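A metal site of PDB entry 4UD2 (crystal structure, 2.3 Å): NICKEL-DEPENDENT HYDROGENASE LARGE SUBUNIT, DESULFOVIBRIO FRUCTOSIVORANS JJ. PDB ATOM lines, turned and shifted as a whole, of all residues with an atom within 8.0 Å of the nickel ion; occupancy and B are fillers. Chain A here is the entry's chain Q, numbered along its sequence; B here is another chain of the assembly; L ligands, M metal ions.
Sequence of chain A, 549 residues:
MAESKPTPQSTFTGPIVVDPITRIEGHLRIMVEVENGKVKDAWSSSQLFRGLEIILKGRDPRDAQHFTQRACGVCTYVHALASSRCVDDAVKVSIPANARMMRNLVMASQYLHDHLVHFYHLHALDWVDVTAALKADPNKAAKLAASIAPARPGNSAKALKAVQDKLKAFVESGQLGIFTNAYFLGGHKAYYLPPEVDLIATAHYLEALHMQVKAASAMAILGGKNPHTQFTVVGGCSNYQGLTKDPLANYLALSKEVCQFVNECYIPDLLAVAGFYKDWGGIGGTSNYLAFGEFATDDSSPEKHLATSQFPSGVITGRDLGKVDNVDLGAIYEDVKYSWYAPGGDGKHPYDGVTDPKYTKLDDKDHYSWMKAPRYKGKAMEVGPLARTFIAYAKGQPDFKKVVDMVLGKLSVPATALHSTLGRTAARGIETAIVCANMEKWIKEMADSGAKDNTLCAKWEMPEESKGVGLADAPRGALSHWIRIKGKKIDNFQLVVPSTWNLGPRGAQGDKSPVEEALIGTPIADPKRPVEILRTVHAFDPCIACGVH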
ATOM      1  N   GLU A  25      25.984  -6.365  25.631  1.00  0.00           N
ATOM      2  CA  GLU A  25      26.270  -4.963  25.437  1.00  0.00           C
ATOM      3  C   GLU A  25      25.742  -4.240  26.684  1.00  0.00           C
ATOM      4  O   GLU A  25      24.572  -4.418  27.069  1.00  0.00           O
ATOM      5  CB  GLU A  25      25.582  -4.456  24.164  1.00  0.00           C
ATOM      6  CG  GLU A  25      25.993  -3.014  23.794  1.00  0.00           C
ATOM      7  CD  GLU A  25      25.664  -2.000  24.908  1.00  0.00           C
ATOM      8  OE1 GLU A  25      24.516  -2.042  25.408  1.00  0.00           O
ATOM      9  OE2 GLU A  25      26.545  -1.162  25.277  1.00  0.00           O
ATOM     10  N   GLN A  69      20.866   6.812  17.032  1.00  0.00           N
ATOM     11  CA  GLN A  69      21.652   5.659  16.540  1.00  0.00           C
ATOM     12  C   GLN A  69      22.710   5.305  17.599  1.00  0.00           C
ATOM     13  O   GLN A  69      23.086   4.153  17.743  1.00  0.00           O
ATOM     14  CB  GLN A  69      22.301   5.908  15.157  1.00  0.00           C
ATOM     15  CG  GLN A  69      22.889   4.614  14.584  1.00  0.00           C
ATOM     16  CD  GLN A  69      23.513   4.719  13.182  1.00  0.00           C
ATOM     17  OE1 GLN A  69      23.860   3.713  12.609  1.00  0.00           O
ATOM     18  NE2 GLN A  69      23.649   5.914  12.645  1.00  0.00           N
ATOM     19  N   ALA A  71      22.312   5.101  20.627  1.00  0.00           N
ATOM     20  CA  ALA A  71      21.739   4.308  21.710  1.00  0.00           C
ATOM     21  C   ALA A  71      22.552   3.012  21.827  1.00  0.00           C
ATOM     22  O   ALA A  71      22.712   2.468  22.929  1.00  0.00           O
ATOM     23  CB  ALA A  71      20.282   3.988  21.436  1.00  0.00           C
ATOM     24  N   CYS A  72      23.056   2.516  20.687  1.00  0.00           N
ATOM     25  CA  CYS A  72      23.755   1.250  20.652  1.00  0.00           C
ATOM     26  C   CYS A  72      24.652   1.081  19.431  1.00  0.00           C
ATOM     27  O   CYS A  72      24.248   1.334  18.275  1.00  0.00           O
ATOM     28  CB  CYS A  72      22.759   0.079  20.689  1.00  0.00           C
ATOM     29  SG  CYS A  72      23.502  -1.581  20.793  1.00  0.00           S
ATOM     30  N   GLY A  73      25.873   0.608  19.676  1.00  0.00           N
ATOM     31  CA  GLY A  73      26.826   0.412  18.607  1.00  0.00           C
ATOM     32  C   GLY A  73      26.881  -1.030  18.189  1.00  0.00           C
ATOM     33  O   GLY A  73      27.535  -1.347  17.203  1.00  0.00           O
ATOM     34  N   VAL A  74      26.208  -1.913  18.939  1.00  0.00           N
ATOM     35  CA  VAL A  74      26.120  -3.330  18.552  1.00  0.00           C
ATOM     36  C   VAL A  74      24.953  -3.509  17.545  1.00  0.00           C
ATOM     37  O   VAL A  74      25.158  -3.985  16.403  1.00  0.00           O
ATOM     38  CB  VAL A  74      25.949  -4.253  19.786  1.00  0.00           C
ATOM     39  CG1 VAL A  74      25.802  -5.712  19.352  1.00  0.00           C
ATOM     40  CG2 VAL A  74      27.154  -4.113  20.717  1.00  0.00           C
ATOM     41  N   CYS A  75      23.748  -3.105  17.958  1.00  0.00           N
ATOM     42  CA  CYS A  75      22.627  -3.081  17.044  1.00  0.00           C
ATOM     43  C   CYS A  75      22.682  -1.716  16.388  1.00  0.00           C
ATOM     44  O   CYS A  75      21.732  -0.926  16.459  1.00  0.00           O
ATOM     45  CB  CYS A  75      21.274  -3.312  17.746  1.00  0.00           C
ATOM     46  SG  CYS A  75      20.832  -2.116  19.028  1.00  0.00           S
ATOM     47  N   THR A  76      23.828  -1.414  15.763  1.00  0.00           N
ATOM     48  CA  THR A  76      23.996  -0.146  15.087  1.00  0.00           C
ATOM     49  C   THR A  76      22.929  -0.122  13.988  1.00  0.00           C
ATOM     50  O   THR A  76      22.322  -1.170  13.672  1.00  0.00           O
ATOM     51  CB  THR A  76      25.440  -0.028  14.541  1.00  0.00           C
ATOM     52  OG1 THR A  76      25.597   1.259  13.954  1.00  0.00           O
ATOM     53  CG2 THR A  76      25.750  -1.136  13.509  1.00  0.00           C
ATOM     54  N   VAL A  78      19.824   0.132  13.484  1.00  0.00           N
ATOM     55  CA  VAL A  78      18.403  -0.040  13.799  1.00  0.00           C
ATOM     56  C   VAL A  78      17.716   1.207  14.356  1.00  0.00           C
ATOM     57  O   VAL A  78      16.580   1.527  13.959  1.00  0.00           O
ATOM     58  CB  VAL A  78      18.152  -1.265  14.697  1.00  0.00           C
ATOM     59  CG1 VAL A  78      18.813  -2.499  14.097  1.00  0.00           C
ATOM     60  CG2 VAL A  78      18.675  -1.038  16.112  1.00  0.00           C
ATOM     61  N   HIS A  79      18.396   1.943  15.246  1.00  0.00           N
ATOM     62  CA  HIS A  79      17.779   3.166  15.788  1.00  0.00           C
ATOM     63  C   HIS A  79      17.690   4.314  14.782  1.00  0.00           C
ATOM     64  O   HIS A  79      16.720   5.097  14.815  1.00  0.00           O
ATOM     65  CB  HIS A  79      18.518   3.630  17.052  1.00  0.00           C
ATOM     66  CG  HIS A  79      18.334   2.714  18.205  1.00  0.00           C
ATOM     67  ND1 HIS A  79      17.134   2.623  18.876  1.00  0.00           N
ATOM     68  CD2 HIS A  79      19.156   1.812  18.770  1.00  0.00           C
ATOM     69  CE1 HIS A  79      17.233   1.704  19.830  1.00  0.00           C
ATOM     70  NE2 HIS A  79      18.448   1.191  19.769  1.00  0.00           N
ATOM     71  N   GLN A 110      22.471  -6.350   8.918  1.00  0.00           N
ATOM     72  CA  GLN A 110      22.645  -6.205  10.382  1.00  0.00           C
ATOM     73  C   GLN A 110      22.273  -7.505  11.109  1.00  0.00           C
ATOM     74  O   GLN A 110      22.983  -7.932  12.003  1.00  0.00           O
ATOM     75  CB  GLN A 110      21.818  -5.034  10.911  1.00  0.00           C
ATOM     76  CG  GLN A 110      21.841  -4.806  12.428  1.00  0.00           C
ATOM     77  CD  GLN A 110      23.251  -4.600  13.025  1.00  0.00           C
ATOM     78  OE1 GLN A 110      24.154  -4.133  12.342  1.00  0.00           O
ATOM     79  NE2 GLN A 110      23.415  -4.946  14.291  1.00  0.00           N
ATOM     80  N   ASP A 114      24.979  -9.308  13.396  1.00  0.00           N
ATOM     81  CA  ASP A 114      24.637  -9.332  14.832  1.00  0.00           C
ATOM     82  C   ASP A 114      24.522 -10.762  15.401  1.00  0.00           C
ATOM     83  O   ASP A 114      25.180 -11.105  16.392  1.00  0.00           O
ATOM     84  CB  ASP A 114      23.327  -8.551  15.034  1.00  0.00           C
ATOM     85  CG  ASP A 114      23.191  -7.931  16.425  1.00  0.00           C
ATOM     86  OD1 ASP A 114      23.602  -8.549  17.423  1.00  0.00           O
ATOM     87  OD2 ASP A 114      22.634  -6.808  16.521  1.00  0.00           O
ATOM     88  N   ALA A 474      14.265  -5.142  15.251  1.00  0.00           N
ATOM     89  CA  ALA A 474      15.728  -5.219  15.298  1.00  0.00           C
ATOM     90  C   ALA A 474      16.142  -6.662  15.606  1.00  0.00           C
ATOM     91  O   ALA A 474      15.296  -7.500  15.925  1.00  0.00           O
ATOM     92  CB  ALA A 474      16.259  -4.252  16.337  1.00  0.00           C
ATOM     93  N   PRO A 475      17.460  -6.966  15.550  1.00  0.00           N
ATOM     94  CA  PRO A 475      17.905  -8.323  15.899  1.00  0.00           C
ATOM     95  C   PRO A 475      17.387  -8.818  17.258  1.00  0.00           C
ATOM     96  O   PRO A 475      17.178 -10.037  17.430  1.00  0.00           O
ATOM     97  CB  PRO A 475      19.430  -8.185  15.893  1.00  0.00           C
ATOM     98  CG  PRO A 475      19.696  -7.113  14.853  1.00  0.00           C
ATOM     99  CD  PRO A 475      18.578  -6.110  15.079  1.00  0.00           C
ATOM    100  N   ARG A 476      17.158  -7.901  18.207  1.00  0.00           N
ATOM    101  CA  ARG A 476      16.700  -8.306  19.541  1.00  0.00           C
ATOM    102  C   ARG A 476      15.211  -8.221  19.762  1.00  0.00           C
ATOM    103  O   ARG A 476      14.735  -8.669  20.796  1.00  0.00           O
ATOM    104  CB  ARG A 476      17.473  -7.560  20.635  1.00  0.00           C
ATOM    105  CG  ARG A 476      18.902  -8.072  20.799  1.00  0.00           C
ATOM    106  CD  ARG A 476      19.839  -7.069  21.431  1.00  0.00           C
ATOM    107  NE  ARG A 476      21.184  -7.611  21.387  1.00  0.00           N
ATOM    108  CZ  ARG A 476      22.025  -7.438  20.374  1.00  0.00           C
ATOM    109  NH1 ARG A 476      21.675  -6.707  19.316  1.00  0.00           N
ATOM    110  NH2 ARG A 476      23.211  -8.033  20.411  1.00  0.00           N
ATOM    111  N   VAL A 497      12.543  -0.073  23.547  1.00  0.00           N
ATOM    112  CA  VAL A 497      13.518  -0.929  22.873  1.00  0.00           C
ATOM    113  C   VAL A 497      13.329  -2.402  23.294  1.00  0.00           C
ATOM    114  O   VAL A 497      12.840  -2.674  24.393  1.00  0.00           O
ATOM    115  CB  VAL A 497      14.955  -0.444  23.138  1.00  0.00           C
ATOM    116  CG1 VAL A 497      15.988  -1.176  22.284  1.00  0.00           C
ATOM    117  CG2 VAL A 497      15.064   1.040  22.858  1.00  0.00           C
ATOM    118  N   PRO A 498      13.690  -3.356  22.407  1.00  0.00           N
ATOM    119  CA  PRO A 498      13.543  -4.769  22.716  1.00  0.00           C
ATOM    120  C   PRO A 498      14.104  -5.188  24.070  1.00  0.00           C
ATOM    121  O   PRO A 498      13.412  -5.845  24.834  1.00  0.00           O
ATOM    122  CB  PRO A 498      14.267  -5.481  21.547  1.00  0.00           C
ATOM    123  CG  PRO A 498      14.824  -4.427  20.687  1.00  0.00           C
ATOM    124  CD  PRO A 498      14.012  -3.183  20.985  1.00  0.00           C
ATOM    125  N   SER A 499      15.342  -4.799  24.385  1.00  0.00           N
ATOM    126  CA  SER A 499      15.898  -5.192  25.680  1.00  0.00           C
ATOM    127  C   SER A 499      15.132  -4.531  26.831  1.00  0.00           C
ATOM    128  O   SER A 499      15.200  -5.010  27.966  1.00  0.00           O
ATOM    129  CB  SER A 499      17.378  -4.888  25.783  1.00  0.00           C
ATOM    130  OG  SER A 499      18.118  -5.657  24.832  1.00  0.00           O
ATOM    131  N   ASP A 541      20.077 -12.225  24.545  1.00  0.00           N
ATOM    132  CA  ASP A 541      20.963 -11.308  23.822  1.00  0.00           C
ATOM    133  C   ASP A 541      20.802  -9.865  24.374  1.00  0.00           C
ATOM    134  O   ASP A 541      20.412  -8.957  23.661  1.00  0.00           O
ATOM    135  CB  ASP A 541      20.649 -11.403  22.311  1.00  0.00           C
ATOM    136  CG  ASP A 541      21.599 -10.613  21.436  1.00  0.00           C
ATOM    137  OD1 ASP A 541      22.650 -10.126  21.907  1.00  0.00           O
ATOM    138  OD2 ASP A 541      21.263 -10.470  20.236  1.00  0.00           O
ATOM    139  N   PRO A 542      21.137  -9.660  25.661  1.00  0.00           N
ATOM    140  CA  PRO A 542      20.872  -8.366  26.317  1.00  0.00           C
ATOM    141  C   PRO A 542      21.682  -7.220  25.726  1.00  0.00           C
ATOM    142  O   PRO A 542      22.863  -7.397  25.420  1.00  0.00           O
ATOM    143  CB  PRO A 542      21.294  -8.606  27.777  1.00  0.00           C
ATOM    144  CG  PRO A 542      21.128 -10.087  27.940  1.00  0.00           C
ATOM    145  CD  PRO A 542      21.664 -10.626  26.635  1.00  0.00           C
ATOM    146  N   CSO A 543      21.025  -6.065  25.578  1.00  0.00           N
ATOM    147  CA  CSO A 543      21.653  -4.814  25.120  1.00  0.00           C
ATOM    148  CB  CSO A 543      21.246  -4.527  23.691  1.00  0.00           C
ATOM    149  SG  CSO A 543      22.374  -3.492  22.821  1.00  0.00           S
ATOM    150  C   CSO A 543      21.186  -3.719  26.056  1.00  0.00           C
ATOM    151  O   CSO A 543      20.095  -3.135  25.861  1.00  0.00           O
ATOM    152  OD  CSO A 543      22.593  -1.884  23.601  1.00  0.00           O
ATOM    153  N   ILE A 544      21.976  -3.431  27.085  1.00  0.00           N
ATOM    154  CA  ILE A 544      21.569  -2.488  28.150  1.00  0.00           C
ATOM    155  C   ILE A 544      21.570  -1.016  27.759  1.00  0.00           C
ATOM    156  O   ILE A 544      20.705  -0.247  28.216  1.00  0.00           O
ATOM    157  CB  ILE A 544      22.400  -2.703  29.440  1.00  0.00           C
ATOM    158  CG1 ILE A 544      22.483  -4.198  29.767  1.00  0.00           C
ATOM    159  CG2 ILE A 544      21.813  -1.937  30.639  1.00  0.00           C
ATOM    160  CD1 ILE A 544      21.144  -4.910  29.871  1.00  0.00           C
ATOM    161  N   ALA A 545      22.529  -0.588  26.941  1.00  0.00           N
ATOM    162  CA  ALA A 545      22.533   0.806  26.456  1.00  0.00           C
ATOM    163  C   ALA A 545      21.232   1.035  25.640  1.00  0.00           C
ATOM    164  O   ALA A 545      20.570   2.066  25.766  1.00  0.00           O
ATOM    165  CB  ALA A 545      23.778   1.104  25.609  1.00  0.00           C
ATOM    166  N   CYS A 546      20.865   0.031  24.825  1.00  0.00           N
ATOM    167  CA  CYS A 546      19.560   0.019  24.130  1.00  0.00           C
ATOM    168  C   CYS A 546      18.429   0.142  25.146  1.00  0.00           C
ATOM    169  O   CYS A 546      17.586   1.047  25.067  1.00  0.00           O
ATOM    170  CB  CYS A 546      19.380  -1.288  23.329  1.00  0.00           C
ATOM    171  SG  CYS A 546      19.827  -1.199  21.599  1.00  0.00           S
ATOM    172  N   GLY A 547      18.408  -0.800  26.083  1.00  0.00           N
ATOM    173  CA  GLY A 547      17.322  -0.868  27.059  1.00  0.00           C
ATOM    174  C   GLY A 547      17.001   0.435  27.779  1.00  0.00           C
ATOM    175  O   GLY A 547      15.828   0.836  27.893  1.00  0.00           O
ATOM    176  N   CYS B  17      28.232   3.166  23.985  1.00  0.00           N
ATOM    177  CA  CYS B  17      27.238   2.431  23.207  1.00  0.00           C
ATOM    178  C   CYS B  17      27.828   1.120  22.691  1.00  0.00           C
ATOM    179  O   CYS B  17      27.130   0.326  22.059  1.00  0.00           O
ATOM    180  CB  CYS B  17      26.738   3.302  22.044  1.00  0.00           C
ATOM    181  SG  CYS B  17      27.797   3.303  20.565  1.00  0.00           S
ATOM    182  N   THR B  18      29.123   0.931  22.973  1.00  0.00           N
ATOM    183  CA  THR B  18      29.899  -0.241  22.544  1.00  0.00           C
ATOM    184  C   THR B  18      30.261  -0.225  21.053  1.00  0.00           C
ATOM    185  O   THR B  18      30.826  -1.191  20.518  1.00  0.00           O
ATOM    186  CB  THR B  18      29.204  -1.553  22.977  1.00  0.00           C
ATOM    187  OG1 THR B  18      28.870  -1.456  24.365  1.00  0.00           O
ATOM    188  CG2 THR B  18      30.106  -2.770  22.792  1.00  0.00           C
HETATM  189 FE1  LIG L   1      19.188  -3.053  20.301  1.00  0.00          FE
HETATM  190  C1  LIG L   1      18.229  -3.861  21.732  1.00  0.00           C
HETATM  191  N1  LIG L   1      17.673  -4.356  22.605  1.00  0.00           N
HETATM  192  C2  LIG L   1      18.826  -4.554  19.208  1.00  0.00           C
HETATM  193  N2  LIG L   1      18.637  -5.431  18.522  1.00  0.00           N
HETATM  194  C3  LIG L   1      17.795  -2.294  19.630  1.00  0.00           C
HETATM  195  O1  LIG L   1      16.876  -1.816  19.148  1.00  0.00           O
HETATM  196 NI    NI M   1      21.649  -2.720  20.918  1.00  0.00          NI
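FE1 of the ligand is bound by SG of Cys 75 (2.3 Å).
SG of Cys 546 binds FE1 of the ligand (2.4 Å).
The backbone NH of Arg 476 is in hydrogen-bond range of a nitrogen (N2) of the ligand, at 2.9 Å.
The guanidinium group (NH1) of Arg 476 sits close to a nitrogen (N2) of the ligand, at 3.4 Å.
A ring nitrogen (NE2) of His 79 sits at hydrogen-bond distance from an oxygen (O1) of the ligand (3.4 Å).
The backbone NH of Ser 499 is in hydrogen-bond range of a nitrogen (N1) of the ligand (3.0 Å).
The side-chain hydroxyl of Ser 499 is in hydrogen-bond range of a nitrogen (N1) of the ligand (2.6 Å).
OD of CSO 543 is in hydrogen-bond range of OE1 of Glu 25, 2.6 Å away.
The side-chain hydroxyl (OG) of Ser 499 is in hydrogen-bond range of N of CSO 543 (3.0 Å).
SG of Cys 72 lies close to N of Val 74, 3.3 Å away.
The side-chain sulfur (SG) of Cys 546 lies close to a ring nitrogen (NE2) of His 79 (3.3 Å).
Of the 27 residues printed, 4 come within 4 Å of the nickel ion.
Along chain A the residues within 4 Å of the nickel ion span positions 72 to 546.
The nearest printed residue that does not touch the nickel ion is Arg 476 (4.3 Å).
The nickel ion is bound by SG of Cys 75 (2.1 Å), SG of CSO 543 (2.2 Å), SG of Cys 72 (2.2 Å) and SG of Cys 546 (2.5 Å).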
